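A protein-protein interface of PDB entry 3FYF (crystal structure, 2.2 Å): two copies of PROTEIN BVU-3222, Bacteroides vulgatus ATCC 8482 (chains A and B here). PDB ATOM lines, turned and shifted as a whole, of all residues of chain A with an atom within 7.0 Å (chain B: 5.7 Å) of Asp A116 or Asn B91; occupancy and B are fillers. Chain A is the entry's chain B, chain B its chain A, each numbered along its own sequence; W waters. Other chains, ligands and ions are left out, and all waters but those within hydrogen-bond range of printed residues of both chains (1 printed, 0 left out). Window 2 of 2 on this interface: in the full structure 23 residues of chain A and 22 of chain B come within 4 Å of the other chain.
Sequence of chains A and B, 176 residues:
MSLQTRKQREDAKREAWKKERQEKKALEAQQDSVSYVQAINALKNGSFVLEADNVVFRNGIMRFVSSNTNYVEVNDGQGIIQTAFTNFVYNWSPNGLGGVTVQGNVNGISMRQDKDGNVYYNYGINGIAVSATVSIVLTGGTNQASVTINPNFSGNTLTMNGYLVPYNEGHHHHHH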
ATOM      1  N   TYR A  36      27.568  11.063 -11.484  1.00  0.00           N
ATOM      2  CA  TYR A  36      28.186  11.316 -12.781  1.00  0.00           C
ATOM      3  C   TYR A  36      29.525  10.602 -12.940  1.00  0.00           C
ATOM      4  O   TYR A  36      29.698   9.836 -13.885  1.00  0.00           O
ATOM      5  CB  TYR A  36      28.352  12.822 -12.991  1.00  0.00           C
ATOM      6  CG  TYR A  36      29.107  13.236 -14.233  1.00  0.00           C
ATOM      7  CD1 TYR A  36      28.639  12.905 -15.503  1.00  0.00           C
ATOM      8  CD2 TYR A  36      30.268  13.996 -14.136  1.00  0.00           C
ATOM      9  CE1 TYR A  36      29.317  13.306 -16.640  1.00  0.00           C
ATOM     10  CE2 TYR A  36      30.958  14.398 -15.271  1.00  0.00           C
ATOM     11  CZ  TYR A  36      30.473  14.049 -16.520  1.00  0.00           C
ATOM     12  OH  TYR A  36      31.144  14.444 -17.645  1.00  0.00           O
ATOM     13  N   GLN A 113      33.000  12.749 -25.723  1.00  0.00           N
ATOM     14  CA  GLN A 113      32.549  13.717 -24.735  1.00  0.00           C
ATOM     15  C   GLN A 113      32.502  15.097 -25.375  1.00  0.00           C
ATOM     16  O   GLN A 113      33.451  15.499 -26.051  1.00  0.00           O
ATOM     17  CB  GLN A 113      33.496  13.707 -23.521  1.00  0.00           C
ATOM     18  CG  GLN A 113      33.101  14.672 -22.406  1.00  0.00           C
ATOM     19  CD  GLN A 113      33.901  14.492 -21.124  1.00  0.00           C
ATOM     20  OE1 GLN A 113      34.300  13.383 -20.768  1.00  0.00           O
ATOM     21  NE2 GLN A 113      34.118  15.592 -20.408  1.00  0.00           N
ATOM     22  N   ASP A 114      31.404  15.824 -25.171  1.00  0.00           N
ATOM     23  CA  ASP A 114      31.323  17.197 -25.677  1.00  0.00           C
ATOM     24  C   ASP A 114      31.989  18.197 -24.727  1.00  0.00           C
ATOM     25  O   ASP A 114      32.648  17.791 -23.771  1.00  0.00           O
ATOM     26  CB  ASP A 114      29.884  17.589 -26.080  1.00  0.00           C
ATOM     27  CG  ASP A 114      28.932  17.787 -24.903  1.00  0.00           C
ATOM     28  OD1 ASP A 114      29.324  17.727 -23.718  1.00  0.00           O
ATOM     29  OD2 ASP A 114      27.742  18.019 -25.195  1.00  0.00           O
ATOM     30  N   LYS A 115      31.818  19.492 -24.983  1.00  0.00           N
ATOM     31  CA  LYS A 115      32.458  20.518 -24.156  1.00  0.00           C
ATOM     32  C   LYS A 115      31.801  20.670 -22.774  1.00  0.00           C
ATOM     33  O   LYS A 115      32.412  21.200 -21.848  1.00  0.00           O
ATOM     34  CB  LYS A 115      32.557  21.861 -24.899  1.00  0.00           C
ATOM     35  CG  LYS A 115      31.258  22.643 -25.033  1.00  0.00           C
ATOM     36  CD  LYS A 115      31.538  24.063 -25.514  1.00  0.00           C
ATOM     37  CE  LYS A 115      30.369  25.007 -25.242  1.00  0.00           C
ATOM     38  NZ  LYS A 115      29.287  24.876 -26.254  1.00  0.00           N
ATOM     39  N   ASP A 116      30.572  20.171 -22.643  1.00  0.00           N
ATOM     40  CA  ASP A 116      29.809  20.271 -21.402  1.00  0.00           C
ATOM     41  C   ASP A 116      29.841  18.975 -20.593  1.00  0.00           C
ATOM     42  O   ASP A 116      29.104  18.816 -19.617  1.00  0.00           O
ATOM     43  CB  ASP A 116      28.366  20.668 -21.709  1.00  0.00           C
ATOM     44  CG  ASP A 116      28.254  22.085 -22.230  1.00  0.00           C
ATOM     45  OD1 ASP A 116      28.641  23.025 -21.503  1.00  0.00           O
ATOM     46  OD2 ASP A 116      27.774  22.257 -23.367  1.00  0.00           O
ATOM     47  N   GLY A 117      30.693  18.048 -21.009  1.00  0.00           N
ATOM     48  CA  GLY A 117      30.817  16.775 -20.321  1.00  0.00           C
ATOM     49  C   GLY A 117      29.661  15.815 -20.523  1.00  0.00           C
ATOM     50  O   GLY A 117      29.509  14.883 -19.744  1.00  0.00           O
ATOM     51  N   ASN A 118      28.847  16.035 -21.559  1.00  0.00           N
ATOM     52  CA  ASN A 118      27.861  15.034 -21.994  1.00  0.00           C
ATOM     53  C   ASN A 118      28.586  13.934 -22.744  1.00  0.00           C
ATOM     54  O   ASN A 118      29.401  14.221 -23.621  1.00  0.00           O
ATOM     55  CB  ASN A 118      26.792  15.637 -22.911  1.00  0.00           C
ATOM     56  CG  ASN A 118      26.117  16.845 -22.316  1.00  0.00           C
ATOM     57  OD1 ASN A 118      25.610  16.804 -21.194  1.00  0.00           O
ATOM     58  ND2 ASN A 118      26.081  17.932 -23.079  1.00  0.00           N
ATOM     59  N   VAL A 119      28.288  12.684 -22.411  1.00  0.00           N
ATOM     60  CA  VAL A 119      29.025  11.538 -22.963  1.00  0.00           C
ATOM     61  C   VAL A 119      28.193  10.757 -23.979  1.00  0.00           C
ATOM     62  O   VAL A 119      27.031  10.450 -23.742  1.00  0.00           O
ATOM     63  CB  VAL A 119      29.521  10.603 -21.844  1.00  0.00           C
ATOM     64  CG1 VAL A 119      30.285   9.386 -22.404  1.00  0.00           C
ATOM     65  CG2 VAL A 119      30.387  11.380 -20.890  1.00  0.00           C
ATOM     66  N   TYR A 120      28.813  10.449 -25.110  1.00  0.00           N
ATOM     67  CA  TYR A 120      28.170   9.727 -26.188  1.00  0.00           C
ATOM     68  C   TYR A 120      28.846   8.370 -26.332  1.00  0.00           C
ATOM     69  O   TYR A 120      29.962   8.270 -26.839  1.00  0.00           O
ATOM     70  CB  TYR A 120      28.213  10.563 -27.479  1.00  0.00           C
ATOM     71  CG  TYR A 120      27.461  11.877 -27.326  1.00  0.00           C
ATOM     72  CD1 TYR A 120      26.133  11.992 -27.735  1.00  0.00           C
ATOM     73  CD2 TYR A 120      28.062  12.989 -26.735  1.00  0.00           C
ATOM     74  CE1 TYR A 120      25.432  13.189 -27.577  1.00  0.00           C
ATOM     75  CE2 TYR A 120      27.364  14.186 -26.565  1.00  0.00           C
ATOM     76  CZ  TYR A 120      26.058  14.277 -26.985  1.00  0.00           C
ATOM     77  OH  TYR A 120      25.381  15.463 -26.820  1.00  0.00           O
ATOM     78  N   THR A 139      23.875  12.630 -19.638  1.00  0.00           N
ATOM     79  CA  THR A 139      23.846  14.057 -19.326  1.00  0.00           C
ATOM     80  C   THR A 139      24.972  14.417 -18.344  1.00  0.00           C
ATOM     81  O   THR A 139      25.085  13.812 -17.283  1.00  0.00           O
ATOM     82  CB  THR A 139      22.465  14.469 -18.754  1.00  0.00           C
ATOM     83  OG1 THR A 139      21.424  14.033 -19.634  1.00  0.00           O
ATOM     84  CG2 THR A 139      22.369  15.974 -18.577  1.00  0.00           C
ATOM     85  N   GLY A 140      25.793  15.398 -18.715  1.00  0.00           N
ATOM     86  CA  GLY A 140      26.929  15.834 -17.902  1.00  0.00           C
ATOM     87  C   GLY A 140      26.553  16.371 -16.532  1.00  0.00           C
ATOM     88  O   GLY A 140      25.581  17.118 -16.395  1.00  0.00           O
ATOM     89  N   GLY A 141      27.313  15.960 -15.516  1.00  0.00           N
ATOM     90  CA  GLY A 141      27.037  16.328 -14.125  1.00  0.00           C
ATOM     91  C   GLY A 141      25.896  15.556 -13.485  1.00  0.00           C
ATOM     92  O   GLY A 141      25.452  15.916 -12.402  1.00  0.00           O
ATOM     93  N   ASN B  59      19.670  16.814 -29.420  1.00  0.00           N
ATOM     94  CA  ASN B  59      20.926  16.073 -29.367  1.00  0.00           C
ATOM     95  C   ASN B  59      20.915  14.826 -28.466  1.00  0.00           C
ATOM     96  O   ASN B  59      21.974  14.327 -28.089  1.00  0.00           O
ATOM     97  CB  ASN B  59      22.088  17.004 -29.001  1.00  0.00           C
ATOM     98  CG  ASN B  59      21.975  17.592 -27.602  1.00  0.00           C
ATOM     99  OD1 ASN B  59      20.938  17.506 -26.939  1.00  0.00           O
ATOM    100  ND2 ASN B  59      23.060  18.211 -27.151  1.00  0.00           N
ATOM    101  N   ILE B  61      19.970  14.347 -25.359  1.00  0.00           N
ATOM    102  CA  ILE B  61      20.061  14.559 -23.914  1.00  0.00           C
ATOM    103  C   ILE B  61      18.674  14.452 -23.302  1.00  0.00           C
ATOM    104  O   ILE B  61      17.728  15.062 -23.799  1.00  0.00           O
ATOM    105  CB  ILE B  61      20.714  15.934 -23.591  1.00  0.00           C
ATOM    106  CG1 ILE B  61      22.224  15.860 -23.811  1.00  0.00           C
ATOM    107  CG2 ILE B  61      20.409  16.419 -22.149  1.00  0.00           C
ATOM    108  CD1 ILE B  61      22.886  17.213 -23.811  1.00  0.00           C
ATOM    109  N   VAL B  89      17.426  24.154 -25.832  1.00  0.00           N
ATOM    110  CA  VAL B  89      18.668  23.377 -25.786  1.00  0.00           C
ATOM    111  C   VAL B  89      19.059  23.279 -24.313  1.00  0.00           C
ATOM    112  O   VAL B  89      18.875  24.240 -23.558  1.00  0.00           O
ATOM    113  CB  VAL B  89      19.826  24.045 -26.615  1.00  0.00           C
ATOM    114  CG1 VAL B  89      21.045  23.133 -26.711  1.00  0.00           C
ATOM    115  CG2 VAL B  89      19.370  24.405 -28.019  1.00  0.00           C
ATOM    116  N   TYR B  90      19.570  22.116 -23.907  1.00  0.00           N
ATOM    117  CA  TYR B  90      19.942  21.858 -22.513  1.00  0.00           C
ATOM    118  C   TYR B  90      21.063  22.770 -22.006  1.00  0.00           C
ATOM    119  O   TYR B  90      20.987  23.306 -20.896  1.00  0.00           O
ATOM    120  CB  TYR B  90      20.344  20.388 -22.322  1.00  0.00           C
ATOM    121  CG  TYR B  90      20.810  20.077 -20.915  1.00  0.00           C
ATOM    122  CD1 TYR B  90      19.905  20.036 -19.857  1.00  0.00           C
ATOM    123  CD2 TYR B  90      22.158  19.836 -20.637  1.00  0.00           C
ATOM    124  CE1 TYR B  90      20.326  19.775 -18.569  1.00  0.00           C
ATOM    125  CE2 TYR B  90      22.586  19.567 -19.337  1.00  0.00           C
ATOM    126  CZ  TYR B  90      21.662  19.533 -18.313  1.00  0.00           C
ATOM    127  OH  TYR B  90      22.057  19.262 -17.025  1.00  0.00           O
ATOM    128  N   ASN B  91      22.097  22.929 -22.826  1.00  0.00           N
ATOM    129  CA  ASN B  91      23.272  23.713 -22.462  1.00  0.00           C
ATOM    130  C   ASN B  91      23.222  25.124 -23.041  1.00  0.00           C
ATOM    131  O   ASN B  91      23.851  26.043 -22.515  1.00  0.00           O
ATOM    132  CB  ASN B  91      24.545  22.992 -22.923  1.00  0.00           C
ATOM    133  CG  ASN B  91      24.783  21.679 -22.185  1.00  0.00           C
ATOM    134  OD1 ASN B  91      24.868  20.614 -22.801  1.00  0.00           O
ATOM    135  ND2 ASN B  91      24.889  21.749 -20.860  1.00  0.00           N
HETATM  136  O   HOH W   1      25.877  19.178 -19.490  1.00  0.00           O
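No position is printed for both chains.
Water W1 lies within hydrogen-bond range of OD1 of Asn A118 (2.9 Å), ND2 of Asn B91 (3.1 Å) and O of Asp A116 (3.2 Å).
OD1 of Asn B91 sits close to OD2 of Asp A116, at 3.4 Å. The side-chain amide oxygen (OD1) of Asn B91 sits at hydrogen-bond distance from the side-chain amide nitrogen (ND2) of Asn A118 (3.0 Å).
Of the printed residues of chain B, Asn A118 touches Ile B61 (3.4 Å) and Asn B91 (3.0 Å). Printed residues of chain B within 4 Å of Tyr A120: Asn B59 (3.6 Å). Of the printed residues of chain B, Thr A139 touches Ile B61 (3.6 Å) and Tyr B90 (3.6 Å). Of the printed residues of chain A, Asn B59 touches Tyr A120 (3.6 Å). Of the printed residues of chain A, Asn B91 touches Asp A116 and Asn A118. The nearest printed residue of chain B that does not touch Asp A116 is Tyr B90 (6.3 Å). The nearest residue of chain A that does not touch Asn B91 is Asp A114 (4.6 Å). The nearest printed residue of chain A that does not touch Asn B59 is Asp A114 (5.1 Å).
The side-chain carboxylate (OD1) of Asp A114 is in hydrogen-bond range of the backbone NH (N) of Asp A116. The side-chain carboxylate of Asp A114 sits at hydrogen-bond distance from the side-chain amide nitrogen of Asn A118, 2.7 Å away. The side-chain amide oxygen of Asn A118 is in hydrogen-bond range of the backbone NH of Gly A140 (2.9 Å).
Of the 12 printed residues of chain A, 4 touch a printed residue of chain B. Hydrophobic or aromatic side chains of chain A that line the printed part of chain B: Tyr A120. Of the 5 printed residues of chain B, 4 touch a printed residue of chain A. Among the printed residues, 6 pairs touch across the chains.
Ile B61 touches Asn A118. Tyr A120 touches Asn B59 (OH to ND2, 3.6 Å). Ile B61 touches Thr A139. Thr A139 touches Tyr B90.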
